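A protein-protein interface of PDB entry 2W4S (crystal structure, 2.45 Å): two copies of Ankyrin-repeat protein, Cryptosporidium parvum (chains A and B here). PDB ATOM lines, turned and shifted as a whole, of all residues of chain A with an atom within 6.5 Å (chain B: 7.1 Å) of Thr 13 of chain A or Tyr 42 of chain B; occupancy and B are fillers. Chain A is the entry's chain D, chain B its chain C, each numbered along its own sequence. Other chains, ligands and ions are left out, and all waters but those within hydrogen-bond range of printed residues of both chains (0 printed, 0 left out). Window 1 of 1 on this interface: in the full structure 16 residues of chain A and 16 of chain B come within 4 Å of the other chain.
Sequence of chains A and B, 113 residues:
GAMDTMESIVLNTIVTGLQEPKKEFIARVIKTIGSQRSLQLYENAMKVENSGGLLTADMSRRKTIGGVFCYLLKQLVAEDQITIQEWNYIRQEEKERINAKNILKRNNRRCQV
Of the printed residues of chain B, Thr 13 of chain A touches Leu 39 (3.6 Å), Tyr 42 (3.7 Å), Glu 43 (3.8 Å) and Met 46 (3.6 Å).
Tyr 42 of chain B touches just these residues of chain A: Thr 13, Tyr 42 and Met 46.
Of the printed residues of chain A, Glu 43 of chain B touches Asn 12 (3.0 Å), Thr 13 (3.8 Å) and Thr 16 (3.2 Å).
Of the printed residues of chain A, Gln 36 of chain B touches Ile 9.
Printed residues of chain B within 4 Å of Gly 17 of chain A: Met 46.
Leu 72 of chain B touches none of the printed residues of chain A.
The nearest printed residue of chain B that does not touch Met 46 of chain A is Thr 16 of chain B (4.1 Å).
Thr 13 of chain A touches Leu 39 of chain B, and with the chains exchanged Leu 39 of chain A touches Thr 13 of chain B.
Thr 13 of chain A touches Tyr 42 of chain B, and with the chains exchanged Tyr 42 of chain A touches Thr 13 of chain B.
Thr 16 of chain A touches Met 46 of chain B, but with the chains exchanged Met 46 of chain A does not touch Thr 16 of chain B (4.1 Å).
Leu 39 of chain B touches its own counterpart, Leu 39 of chain A.
The backbone carbonyl oxygen (O) of Gln 40 of chain B lies within hydrogen-bond range of the side-chain amide nitrogen (ND2) of Asn 44 of chain B (2.8 Å).
The side-chain hydroxyl (OH) of Tyr 42 of chain B is in hydrogen-bond range of the side-chain sulfur (SD) of Met 46 of chain B (3.5 Å).
The side-chain carboxylate (OE2) of Glu 43 of chain B is in salt-bridge range of the side-chain amino group (NZ) of Lys 47 of chain B, 3.7 Å away.
O of Ser 8 of chain A sits at hydrogen-bond distance from ND2 of Asn 12 of chain A (2.6 Å).
The backbone carbonyl oxygen (O) of Ile 9 of chain A lies within hydrogen-bond range of the side-chain hydroxyl (OG1) of Thr 13 of chain A (3.1 Å).
The side-chain hydroxyl of Thr 16 of chain A is in hydrogen-bond range of the backbone carbonyl oxygen of Asn 12 of chain A, at 2.9 Å.
Of the 14 printed residues of chain A, 8 touch a printed residue of chain B.
Printed residues of chain A that touch a printed residue of chain B: Ile 9, Asn 12, Thr 13, Thr 16, Gly 17, Leu 39, Tyr 42 and Met 46.
Hydrophobic or aromatic side chains of chain B within 4 Å of the printed part of chain A: Leu 39, Tyr 42 and Met 46.
Among the printed residues, no Asp or Glu carboxylate lies within 4 Å of a Lys or Arg side-chain nitrogen of the other chain.
Among the printed residues, pairs that only touch across the chains: Ile 9 of chain A with Gln 40 of chain B, Met 46 of chain A with Thr 13 of chain B, Thr 13 of chain A with Met 46 of chain B, Gly 17 of chain A with Met 46 of chain B, Thr 13 of chain A with Leu 39 of chain B, Met 46 of chain A with Gly 17 of chain B, Ile 9 of chain A with Gln 36 of chain B, Thr 16 of chain A with Met 46 of chain B, Thr 13 of chain A with Tyr 42 of chain B, Ile 9 of chain A with Leu 39 of chain B, Thr 16 of chain A with Lys 47 of chain B, Leu 39 of chain A with Thr 13 of chain B, Thr 13 of chain A with Glu 43 of chain B, Tyr 42 of chain A with Thr 13 of chain B and Leu 39 of chain A with Leu 39 of chain B.
OH of Tyr 42 of chain B lies within hydrogen-bond range of OH of Tyr 42 of chain A (3.0 Å).
SD of Met 46 of chain A sits at hydrogen-bond distance from OH of Tyr 42 of chain B.
The side-chain hydroxyl (OG1) of Thr 16 of chain A sits at hydrogen-bond distance from the side-chain carboxylate (OE2) of Glu 43 of chain B (3.2 Å).
The side-chain sulfur (SD) of Met 46 of chain B sits at hydrogen-bond distance from the side-chain hydroxyl (OH) of Tyr 42 of chain A (3.1 Å).
The side-chain carboxylate of Glu 43 of chain B lies close to the backbone carbonyl oxygen of Asn 12 of chain A (3.3 Å).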
ATOM      1  N   SER A   8      -2.883  -6.331  -1.799  1.00  0.00           N
ATOM      2  CA  SER A   8      -2.595  -5.473  -0.652  1.00  0.00           C
ATOM      3  C   SER A   8      -3.233  -4.097  -0.816  1.00  0.00           C
ATOM      4  O   SER A   8      -3.501  -3.403   0.157  1.00  0.00           O
ATOM      5  CB  SER A   8      -1.095  -5.296  -0.479  1.00  0.00           C
ATOM      6  OG  SER A   8      -0.818  -4.532   0.676  1.00  0.00           O
ATOM      7  N   ILE A   9      -3.468  -3.702  -2.056  1.00  0.00           N
ATOM      8  CA  ILE A   9      -4.105  -2.424  -2.343  1.00  0.00           C
ATOM      9  C   ILE A   9      -5.639  -2.548  -2.386  1.00  0.00           C
ATOM     10  O   ILE A   9      -6.351  -1.635  -1.937  1.00  0.00           O
ATOM     11  CB  ILE A   9      -3.499  -1.795  -3.618  1.00  0.00           C
ATOM     12  CG1 ILE A   9      -2.173  -1.119  -3.247  1.00  0.00           C
ATOM     13  CG2 ILE A   9      -4.430  -0.787  -4.246  1.00  0.00           C
ATOM     14  CD1 ILE A   9      -1.133  -1.230  -4.282  1.00  0.00           C
ATOM     15  N   VAL A  10      -6.141  -3.668  -2.912  1.00  0.00           N
ATOM     16  CA  VAL A  10      -7.560  -3.947  -2.858  1.00  0.00           C
ATOM     17  C   VAL A  10      -7.950  -4.018  -1.374  1.00  0.00           C
ATOM     18  O   VAL A  10      -8.892  -3.357  -0.955  1.00  0.00           O
ATOM     19  CB  VAL A  10      -7.923  -5.230  -3.619  1.00  0.00           C
ATOM     20  CG1 VAL A  10      -9.391  -5.544  -3.477  1.00  0.00           C
ATOM     21  CG2 VAL A  10      -7.591  -5.086  -5.074  1.00  0.00           C
ATOM     22  N   LEU A  11      -7.177  -4.759  -0.580  1.00  0.00           N
ATOM     23  CA  LEU A  11      -7.345  -4.788   0.875  1.00  0.00           C
ATOM     24  C   LEU A  11      -7.568  -3.412   1.481  1.00  0.00           C
ATOM     25  O   LEU A  11      -8.563  -3.192   2.169  1.00  0.00           O
ATOM     26  CB  LEU A  11      -6.158  -5.488   1.566  1.00  0.00           C
ATOM     27  CG  LEU A  11      -6.194  -5.736   3.091  1.00  0.00           C
ATOM     28  CD1 LEU A  11      -7.541  -6.287   3.600  1.00  0.00           C
ATOM     29  CD2 LEU A  11      -5.034  -6.640   3.562  1.00  0.00           C
ATOM     30  N   ASN A  12      -6.654  -2.485   1.225  1.00  0.00           N
ATOM     31  CA  ASN A  12      -6.719  -1.186   1.873  1.00  0.00           C
ATOM     32  C   ASN A  12      -7.829  -0.336   1.304  1.00  0.00           C
ATOM     33  O   ASN A  12      -8.434   0.431   2.036  1.00  0.00           O
ATOM     34  CB  ASN A  12      -5.392  -0.431   1.775  1.00  0.00           C
ATOM     35  CG  ASN A  12      -4.306  -1.000   2.689  1.00  0.00           C
ATOM     36  OD1 ASN A  12      -4.285  -0.752   3.897  1.00  0.00           O
ATOM     37  ND2 ASN A  12      -3.376  -1.739   2.099  1.00  0.00           N
ATOM     38  N   THR A  13      -8.093  -0.451   0.007  1.00  0.00           N
ATOM     39  CA  THR A  13      -9.201   0.301  -0.584  1.00  0.00           C
ATOM     40  C   THR A  13     -10.516  -0.099   0.099  1.00  0.00           C
ATOM     41  O   THR A  13     -11.226   0.739   0.650  1.00  0.00           O
ATOM     42  CB  THR A  13      -9.305   0.094  -2.124  1.00  0.00           C
ATOM     43  OG1 THR A  13      -8.202   0.745  -2.755  1.00  0.00           O
ATOM     44  CG2 THR A  13     -10.598   0.688  -2.688  1.00  0.00           C
ATOM     45  N   ILE A  14     -10.795  -1.391   0.100  1.00  0.00           N
ATOM     46  CA  ILE A  14     -12.049  -1.886   0.634  1.00  0.00           C
ATOM     47  C   ILE A  14     -12.176  -1.591   2.129  1.00  0.00           C
ATOM     48  O   ILE A  14     -13.253  -1.157   2.576  1.00  0.00           O
ATOM     49  CB  ILE A  14     -12.244  -3.378   0.334  1.00  0.00           C
ATOM     50  CG1 ILE A  14     -12.229  -3.612  -1.172  1.00  0.00           C
ATOM     51  CG2 ILE A  14     -13.550  -3.895   0.938  1.00  0.00           C
ATOM     52  CD1 ILE A  14     -12.293  -5.075  -1.522  1.00  0.00           C
ATOM     53  N   VAL A  15     -11.091  -1.800   2.883  1.00  0.00           N
ATOM     54  CA  VAL A  15     -11.063  -1.476   4.324  1.00  0.00           C
ATOM     55  C   VAL A  15     -11.336   0.016   4.577  1.00  0.00           C
ATOM     56  O   VAL A  15     -12.192   0.377   5.389  1.00  0.00           O
ATOM     57  CB  VAL A  15      -9.736  -1.952   5.021  1.00  0.00           C
ATOM     58  CG1 VAL A  15      -9.453  -1.166   6.295  1.00  0.00           C
ATOM     59  CG2 VAL A  15      -9.791  -3.442   5.334  1.00  0.00           C
ATOM     60  N   THR A  16     -10.624   0.886   3.867  1.00  0.00           N
ATOM     61  CA  THR A  16     -10.884   2.331   3.943  1.00  0.00           C
ATOM     62  C   THR A  16     -12.348   2.687   3.621  1.00  0.00           C
ATOM     63  O   THR A  16     -12.956   3.473   4.337  1.00  0.00           O
ATOM     64  CB  THR A  16      -9.886   3.128   3.051  1.00  0.00           C
ATOM     65  OG1 THR A  16      -8.554   2.879   3.516  1.00  0.00           O
ATOM     66  CG2 THR A  16     -10.158   4.654   3.087  1.00  0.00           C
ATOM     67  N   GLY A  17     -12.910   2.084   2.575  1.00  0.00           N
ATOM     68  CA  GLY A  17     -14.237   2.456   2.101  1.00  0.00           C
ATOM     69  C   GLY A  17     -15.351   1.928   2.978  1.00  0.00           C
ATOM     70  O   GLY A  17     -16.413   2.536   3.088  1.00  0.00           O
ATOM     71  N   LEU A  18     -15.094   0.773   3.588  1.00  0.00           N
ATOM     72  CA  LEU A  18     -15.981   0.172   4.587  1.00  0.00           C
ATOM     73  C   LEU A  18     -15.828   0.812   5.957  1.00  0.00           C
ATOM     74  O   LEU A  18     -16.722   0.661   6.794  1.00  0.00           O
ATOM     75  CB  LEU A  18     -15.686  -1.312   4.709  1.00  0.00           C
ATOM     76  CG  LEU A  18     -16.511  -2.301   3.887  1.00  0.00           C
ATOM     77  CD1 LEU A  18     -17.318  -1.688   2.749  1.00  0.00           C
ATOM     78  CD2 LEU A  18     -15.648  -3.423   3.383  1.00  0.00           C
ATOM     79  N   LEU A  39     -13.583  -6.564  -5.262  1.00  0.00           N
ATOM     80  CA  LEU A  39     -13.882  -5.194  -5.655  1.00  0.00           C
ATOM     81  C   LEU A  39     -15.281  -5.082  -6.234  1.00  0.00           C
ATOM     82  O   LEU A  39     -16.013  -4.138  -5.928  1.00  0.00           O
ATOM     83  CB  LEU A  39     -12.870  -4.667  -6.664  1.00  0.00           C
ATOM     84  CG  LEU A  39     -11.509  -4.210  -6.136  1.00  0.00           C
ATOM     85  CD1 LEU A  39     -10.554  -4.012  -7.285  1.00  0.00           C
ATOM     86  CD2 LEU A  39     -11.653  -2.945  -5.277  1.00  0.00           C
ATOM     87  N   TYR A  42     -17.446  -4.986  -3.303  1.00  0.00           N
ATOM     88  CA  TYR A  42     -17.313  -3.677  -2.672  1.00  0.00           C
ATOM     89  C   TYR A  42     -18.060  -2.657  -3.494  1.00  0.00           C
ATOM     90  O   TYR A  42     -18.833  -1.877  -2.958  1.00  0.00           O
ATOM     91  CB  TYR A  42     -15.853  -3.258  -2.531  1.00  0.00           C
ATOM     92  CG  TYR A  42     -15.654  -1.795  -2.176  1.00  0.00           C
ATOM     93  CD1 TYR A  42     -16.044  -1.291  -0.933  1.00  0.00           C
ATOM     94  CD2 TYR A  42     -15.069  -0.899  -3.091  1.00  0.00           C
ATOM     95  CE1 TYR A  42     -15.857   0.062  -0.599  1.00  0.00           C
ATOM     96  CE2 TYR A  42     -14.872   0.456  -2.764  1.00  0.00           C
ATOM     97  CZ  TYR A  42     -15.270   0.925  -1.518  1.00  0.00           C
ATOM     98  OH  TYR A  42     -15.099   2.253  -1.204  1.00  0.00           O
ATOM     99  N   MET A  46     -21.593  -0.505  -2.548  1.00  0.00           N
ATOM    100  CA  MET A  46     -21.639   0.943  -2.686  1.00  0.00           C
ATOM    101  C   MET A  46     -22.921   1.363  -3.389  1.00  0.00           C
ATOM    102  O   MET A  46     -23.618   2.267  -2.917  1.00  0.00           O
ATOM    103  CB  MET A  46     -20.420   1.464  -3.473  1.00  0.00           C
ATOM    104  CG  MET A  46     -19.198   1.805  -2.638  1.00  0.00           C
ATOM    105  SD  MET A  46     -17.968   2.841  -3.516  1.00  0.00           S
ATOM    106  CE  MET A  46     -17.390   1.747  -4.818  1.00  0.00           C
ATOM    107  N   VAL B  10     -11.533  -2.029 -11.764  1.00  0.00           N
ATOM    108  CA  VAL B  10     -10.977  -0.868 -11.083  1.00  0.00           C
ATOM    109  C   VAL B  10     -11.691   0.392 -11.596  1.00  0.00           C
ATOM    110  O   VAL B  10     -12.146   1.220 -10.802  1.00  0.00           O
ATOM    111  CB  VAL B  10      -9.443  -0.822 -11.233  1.00  0.00           C
ATOM    112  CG1 VAL B  10      -8.854   0.426 -10.604  1.00  0.00           C
ATOM    113  CG2 VAL B  10      -8.841  -2.058 -10.578  1.00  0.00           C
ATOM    114  N   THR B  13     -15.276   0.490 -10.122  1.00  0.00           N
ATOM    115  CA  THR B  13     -15.162   0.788  -8.706  1.00  0.00           C
ATOM    116  C   THR B  13     -14.869   2.275  -8.477  1.00  0.00           C
ATOM    117  O   THR B  13     -15.560   2.924  -7.680  1.00  0.00           O
ATOM    118  CB  THR B  13     -14.071  -0.041  -8.065  1.00  0.00           C
ATOM    119  OG1 THR B  13     -14.451  -1.418  -8.116  1.00  0.00           O
ATOM    120  CG2 THR B  13     -13.828   0.383  -6.602  1.00  0.00           C
ATOM    121  N   ILE B  14     -13.848   2.808  -9.153  1.00  0.00           N
ATOM    122  CA  ILE B  14     -13.471   4.203  -8.955  1.00  0.00           C
ATOM    123  C   ILE B  14     -14.616   5.103  -9.447  1.00  0.00           C
ATOM    124  O   ILE B  14     -15.002   6.070  -8.772  1.00  0.00           O
ATOM    125  CB  ILE B  14     -12.135   4.544  -9.688  1.00  0.00           C
ATOM    126  CG1 ILE B  14     -11.001   3.617  -9.184  1.00  0.00           C
ATOM    127  CG2 ILE B  14     -11.783   6.002  -9.541  1.00  0.00           C
ATOM    128  CD1 ILE B  14      -9.652   3.902  -9.767  1.00  0.00           C
ATOM    129  N   VAL B  15     -15.171   4.765 -10.616  1.00  0.00           N
ATOM    130  CA  VAL B  15     -16.260   5.553 -11.191  1.00  0.00           C
ATOM    131  C   VAL B  15     -17.450   5.650 -10.232  1.00  0.00           C
ATOM    132  O   VAL B  15     -17.946   6.754  -9.978  1.00  0.00           O
ATOM    133  CB  VAL B  15     -16.693   5.031 -12.595  1.00  0.00           C
ATOM    134  CG1 VAL B  15     -18.039   5.595 -13.005  1.00  0.00           C
ATOM    135  CG2 VAL B  15     -15.638   5.384 -13.649  1.00  0.00           C
ATOM    136  N   THR B  16     -17.889   4.508  -9.688  1.00  0.00           N
ATOM    137  CA  THR B  16     -18.969   4.477  -8.712  1.00  0.00           C
ATOM    138  C   THR B  16     -18.578   5.176  -7.408  1.00  0.00           C
ATOM    139  O   THR B  16     -19.364   5.903  -6.827  1.00  0.00           O
ATOM    140  CB  THR B  16     -19.392   3.030  -8.406  1.00  0.00           C
ATOM    141  OG1 THR B  16     -19.937   2.423  -9.584  1.00  0.00           O
ATOM    142  CG2 THR B  16     -20.437   2.979  -7.267  1.00  0.00           C
ATOM    143  N   GLY B  17     -17.360   4.951  -6.953  1.00  0.00           N
ATOM    144  CA  GLY B  17     -16.896   5.550  -5.724  1.00  0.00           C
ATOM    145  C   GLY B  17     -16.800   7.062  -5.747  1.00  0.00           C
ATOM    146  O   GLY B  17     -17.050   7.699  -4.730  1.00  0.00           O
ATOM    147  N   LEU B  18     -16.438   7.641  -6.891  1.00  0.00           N
ATOM    148  CA  LEU B  18     -16.386   9.101  -7.033  1.00  0.00           C
ATOM    149  C   LEU B  18     -17.675   9.767  -7.556  1.00  0.00           C
ATOM    150  O   LEU B  18     -17.760  10.998  -7.575  1.00  0.00           O
ATOM    151  CB  LEU B  18     -15.234   9.499  -7.943  1.00  0.00           C
ATOM    152  CG  LEU B  18     -13.849   8.943  -7.619  1.00  0.00           C
ATOM    153  CD1 LEU B  18     -12.968   9.273  -8.802  1.00  0.00           C
ATOM    154  CD2 LEU B  18     -13.290   9.490  -6.269  1.00  0.00           C
ATOM    155  N   GLN B  36      -3.328  -0.256 -10.445  1.00  0.00           N
ATOM    156  CA  GLN B  36      -2.685  -0.225  -9.151  1.00  0.00           C
ATOM    157  C   GLN B  36      -2.576   1.192  -8.571  1.00  0.00           C
ATOM    158  O   GLN B  36      -3.073   1.431  -7.483  1.00  0.00           O
ATOM    159  CB  GLN B  36      -1.326  -0.910  -9.236  1.00  0.00           C
ATOM    160  CG  GLN B  36      -0.803  -1.463  -7.931  1.00  0.00           C
ATOM    161  CD  GLN B  36       0.222  -2.562  -8.153  1.00  0.00           C
ATOM    162  OE1 GLN B  36      -0.120  -3.683  -8.545  1.00  0.00           O
ATOM    163  NE2 GLN B  36       1.487  -2.247  -7.902  1.00  0.00           N
ATOM    164  N   ARG B  37      -1.959   2.142  -9.272  1.00  0.00           N
ATOM    165  CA  ARG B  37      -1.791   3.502  -8.705  1.00  0.00           C
ATOM    166  C   ARG B  37      -3.121   4.272  -8.645  1.00  0.00           C
ATOM    167  O   ARG B  37      -3.343   5.068  -7.728  1.00  0.00           O
ATOM    168  CB  ARG B  37      -0.680   4.303  -9.437  1.00  0.00           C
ATOM    169  CG  ARG B  37       0.745   3.698  -9.284  1.00  0.00           C
ATOM    170  CD  ARG B  37       1.753   4.321 -10.255  1.00  0.00           C
ATOM    171  NE  ARG B  37       2.614   5.348  -9.645  1.00  0.00           N
ATOM    172  CZ  ARG B  37       3.929   5.197  -9.428  1.00  0.00           C
ATOM    173  NH1 ARG B  37       4.549   4.064  -9.780  1.00  0.00           N
ATOM    174  NH2 ARG B  37       4.636   6.177  -8.865  1.00  0.00           N
ATOM    175  N   SER B  38      -3.994   4.018  -9.621  1.00  0.00           N
ATOM    176  CA  SER B  38      -5.369   4.519  -9.631  1.00  0.00           C
ATOM    177  C   SER B  38      -6.157   4.175  -8.344  1.00  0.00           C
ATOM    178  O   SER B  38      -6.790   5.051  -7.744  1.00  0.00           O
ATOM    179  CB  SER B  38      -6.099   3.960 -10.832  1.00  0.00           C
ATOM    180  OG  SER B  38      -5.610   4.553 -12.008  1.00  0.00           O
ATOM    181  N   LEU B  39      -6.094   2.913  -7.916  1.00  0.00           N
ATOM    182  CA  LEU B  39      -6.787   2.495  -6.702  1.00  0.00           C
ATOM    183  C   LEU B  39      -6.244   3.185  -5.463  1.00  0.00           C
ATOM    184  O   LEU B  39      -7.024   3.618  -4.608  1.00  0.00           O
ATOM    185  CB  LEU B  39      -6.771   0.970  -6.522  1.00  0.00           C
ATOM    186  CG  LEU B  39      -8.006   0.139  -6.894  1.00  0.00           C
ATOM    187  CD1 LEU B  39      -7.800  -1.314  -6.473  1.00  0.00           C
ATOM    188  CD2 LEU B  39      -9.289   0.680  -6.263  1.00  0.00           C
ATOM    189  N   GLN B  40      -4.922   3.300  -5.381  1.00  0.00           N
ATOM    190  CA  GLN B  40      -4.244   4.060  -4.304  1.00  0.00           C
ATOM    191  C   GLN B  40      -4.703   5.505  -4.238  1.00  0.00           C
ATOM    192  O   GLN B  40      -4.830   6.057  -3.145  1.00  0.00           O
ATOM    193  CB  GLN B  40      -2.721   4.042  -4.448  1.00  0.00           C
ATOM    194  CG  GLN B  40      -2.046   2.769  -3.960  1.00  0.00           C
ATOM    195  CD  GLN B  40      -0.513   2.775  -4.156  1.00  0.00           C
ATOM    196  OE1 GLN B  40       0.100   1.740  -4.479  1.00  0.00           O
ATOM    197  NE2 GLN B  40       0.104   3.945  -3.964  1.00  0.00           N
ATOM    198  N   LEU B  41      -4.943   6.113  -5.399  1.00  0.00           N
ATOM    199  CA  LEU B  41      -5.468   7.485  -5.462  1.00  0.00           C
ATOM    200  C   LEU B  41      -6.929   7.562  -4.927  1.00  0.00           C
ATOM    201  O   LEU B  41      -7.308   8.512  -4.228  1.00  0.00           O
ATOM    202  CB  LEU B  41      -5.391   7.973  -6.907  1.00  0.00           C
ATOM    203  CG  LEU B  41      -5.183   9.424  -7.314  1.00  0.00           C
ATOM    204  CD1 LEU B  41      -3.964  10.070  -6.622  1.00  0.00           C
ATOM    205  CD2 LEU B  41      -4.993   9.421  -8.805  1.00  0.00           C
ATOM    206  N   TYR B  42      -7.733   6.555  -5.280  1.00  0.00           N
ATOM    207  CA  TYR B  42      -9.140   6.474  -4.877  1.00  0.00           C
ATOM    208  C   TYR B  42      -9.199   6.311  -3.368  1.00  0.00           C
ATOM    209  O   TYR B  42      -9.916   7.035  -2.672  1.00  0.00           O
ATOM    210  CB  TYR B  42      -9.834   5.322  -5.612  1.00  0.00           C
ATOM    211  CG  TYR B  42     -11.193   4.971  -5.072  1.00  0.00           C
ATOM    212  CD1 TYR B  42     -12.167   5.940  -4.942  1.00  0.00           C
ATOM    213  CD2 TYR B  42     -11.506   3.668  -4.697  1.00  0.00           C
ATOM    214  CE1 TYR B  42     -13.399   5.644  -4.439  1.00  0.00           C
ATOM    215  CE2 TYR B  42     -12.775   3.343  -4.184  1.00  0.00           C
ATOM    216  CZ  TYR B  42     -13.708   4.341  -4.063  1.00  0.00           C
ATOM    217  OH  TYR B  42     -14.957   4.089  -3.590  1.00  0.00           O
ATOM    218  N   GLU B  43      -8.371   5.394  -2.873  1.00  0.00           N
ATOM    219  CA  GLU B  43      -8.214   5.172  -1.446  1.00  0.00           C
ATOM    220  C   GLU B  43      -7.802   6.421  -0.691  1.00  0.00           C
ATOM    221  O   GLU B  43      -8.386   6.724   0.374  1.00  0.00           O
ATOM    222  CB  GLU B  43      -7.189   4.088  -1.165  1.00  0.00           C
ATOM    223  CG  GLU B  43      -7.065   3.872   0.312  1.00  0.00           C
ATOM    224  CD  GLU B  43      -5.858   3.073   0.705  1.00  0.00           C
ATOM    225  OE1 GLU B  43      -4.900   2.949  -0.108  1.00  0.00           O
ATOM    226  OE2 GLU B  43      -5.883   2.564   1.853  1.00  0.00           O
ATOM    227  N   ASN B  44      -6.799   7.130  -1.225  1.00  0.00           N
ATOM    228  CA  ASN B  44      -6.278   8.340  -0.597  1.00  0.00           C
ATOM    229  C   ASN B  44      -7.312   9.426  -0.534  1.00  0.00           C
ATOM    230  O   ASN B  44      -7.392  10.127   0.463  1.00  0.00           O
ATOM    231  CB  ASN B  44      -5.015   8.832  -1.295  1.00  0.00           C
ATOM    232  CG  ASN B  44      -3.804   7.964  -0.986  1.00  0.00           C
ATOM    233  OD1 ASN B  44      -3.675   7.435   0.122  1.00  0.00           O
ATOM    234  ND2 ASN B  44      -2.927   7.776  -1.975  1.00  0.00           N
ATOM    235  N   ALA B  45      -8.111   9.544  -1.596  1.00  0.00           N
ATOM    236  CA  ALA B  45      -9.253  10.473  -1.658  1.00  0.00           C
ATOM    237  C   ALA B  45     -10.257  10.119  -0.592  1.00  0.00           C
ATOM    238  O   ALA B  45     -10.821  11.010   0.050  1.00  0.00           O
ATOM    239  CB  ALA B  45      -9.925  10.435  -3.024  1.00  0.00           C
ATOM    240  N   MET B  46     -10.483   8.813  -0.409  1.00  0.00           N
ATOM    241  CA  MET B  46     -11.372   8.320   0.666  1.00  0.00           C
ATOM    242  C   MET B  46     -10.833   8.644   2.048  1.00  0.00           C
ATOM    243  O   MET B  46     -11.607   9.025   2.909  1.00  0.00           O
ATOM    244  CB  MET B  46     -11.666   6.827   0.525  1.00  0.00           C
ATOM    245  CG  MET B  46     -12.793   6.495  -0.467  1.00  0.00           C
ATOM    246  SD  MET B  46     -13.329   4.751  -0.526  1.00  0.00           S
ATOM    247  CE  MET B  46     -11.785   3.905  -0.962  1.00  0.00           C
ATOM    248  N   LYS B  47      -9.514   8.528   2.252  1.00  0.00           N
ATOM    249  CA  LYS B  47      -8.894   8.835   3.577  1.00  0.00           C
ATOM    250  C   LYS B  47      -9.063  10.288   3.948  1.00  0.00           C
ATOM    251  O   LYS B  47      -9.424  10.615   5.101  1.00  0.00           O
ATOM    252  CB  LYS B  47      -7.410   8.493   3.622  1.00  0.00           C
ATOM    253  CG  LYS B  47      -7.154   7.023   3.598  1.00  0.00           C
ATOM    254  CD  LYS B  47      -5.718   6.688   3.851  1.00  0.00           C
ATOM    255  CE  LYS B  47      -5.590   5.166   3.820  1.00  0.00           C
ATOM    256  NZ  LYS B  47      -4.314   4.687   4.404  1.00  0.00           N
ATOM    257  N   VAL B  48      -8.832  11.142   2.957  1.00  0.00           N
ATOM    258  CA  VAL B  48      -9.097  12.568   3.057  1.00  0.00           C
ATOM    259  C   VAL B  48     -10.563  12.834   3.387  1.00  0.00           C
ATOM    260  O   VAL B  48     -10.862  13.670   4.247  1.00  0.00           O
ATOM    261  CB  VAL B  48      -8.692  13.348   1.746  1.00  0.00           C
ATOM    262  CG1 VAL B  48      -9.100  14.796   1.857  1.00  0.00           C
ATOM    263  CG2 VAL B  48      -7.205  13.265   1.501  1.00  0.00           C
ATOM    264  N   ILE B  65     -15.851  14.353  -3.455  1.00  0.00           N
ATOM    265  CA  ILE B  65     -14.746  13.406  -3.491  1.00  0.00           C
ATOM    266  C   ILE B  65     -14.145  13.346  -4.907  1.00  0.00           C
ATOM    267  O   ILE B  65     -12.945  13.069  -5.085  1.00  0.00           O
ATOM    268  CB  ILE B  65     -15.163  12.008  -2.912  1.00  0.00           C
ATOM    269  CG1 ILE B  65     -14.026  10.981  -3.032  1.00  0.00           C
ATOM    270  CG2 ILE B  65     -16.463  11.505  -3.546  1.00  0.00           C
ATOM    271  CD1 ILE B  65     -14.252   9.708  -2.170  1.00  0.00           C
ATOM    272  N   PHE B  69     -10.009  13.816  -5.530  1.00  0.00           N
ATOM    273  CA  PHE B  69      -9.277  12.928  -6.440  1.00  0.00           C
ATOM    274  C   PHE B  69      -8.535  13.735  -7.517  1.00  0.00           C
ATOM    275  O   PHE B  69      -7.397  13.412  -7.866  1.00  0.00           O
ATOM    276  CB  PHE B  69     -10.290  11.939  -7.044  1.00  0.00           C
ATOM    277  CG  PHE B  69      -9.693  10.873  -7.928  1.00  0.00           C
ATOM    278  CD1 PHE B  69      -9.291   9.648  -7.390  1.00  0.00           C
ATOM    279  CD2 PHE B  69      -9.577  11.073  -9.308  1.00  0.00           C
ATOM    280  CE1 PHE B  69      -8.769   8.647  -8.211  1.00  0.00           C
ATOM    281  CE2 PHE B  69      -9.039  10.078 -10.143  1.00  0.00           C
ATOM    282  CZ  PHE B  69      -8.642   8.856  -9.591  1.00  0.00           C
ATOM    283  N   LEU B  72      -5.582  15.444  -5.842  1.00  0.00           N
ATOM    284  CA  LEU B  72      -4.568  14.418  -5.584  1.00  0.00           C
ATOM    285  C   LEU B  72      -3.796  13.997  -6.836  1.00  0.00           C
ATOM    286  O   LEU B  72      -2.615  13.690  -6.777  1.00  0.00           O
ATOM    287  CB  LEU B  72      -5.257  13.213  -4.994  1.00  0.00           C
ATOM    288  CG  LEU B  72      -5.032  12.877  -3.527  1.00  0.00           C
ATOM    289  CD1 LEU B  72      -4.471  14.048  -2.736  1.00  0.00           C
ATOM    290  CD2 LEU B  72      -6.304  12.260  -2.898  1.00  0.00           C
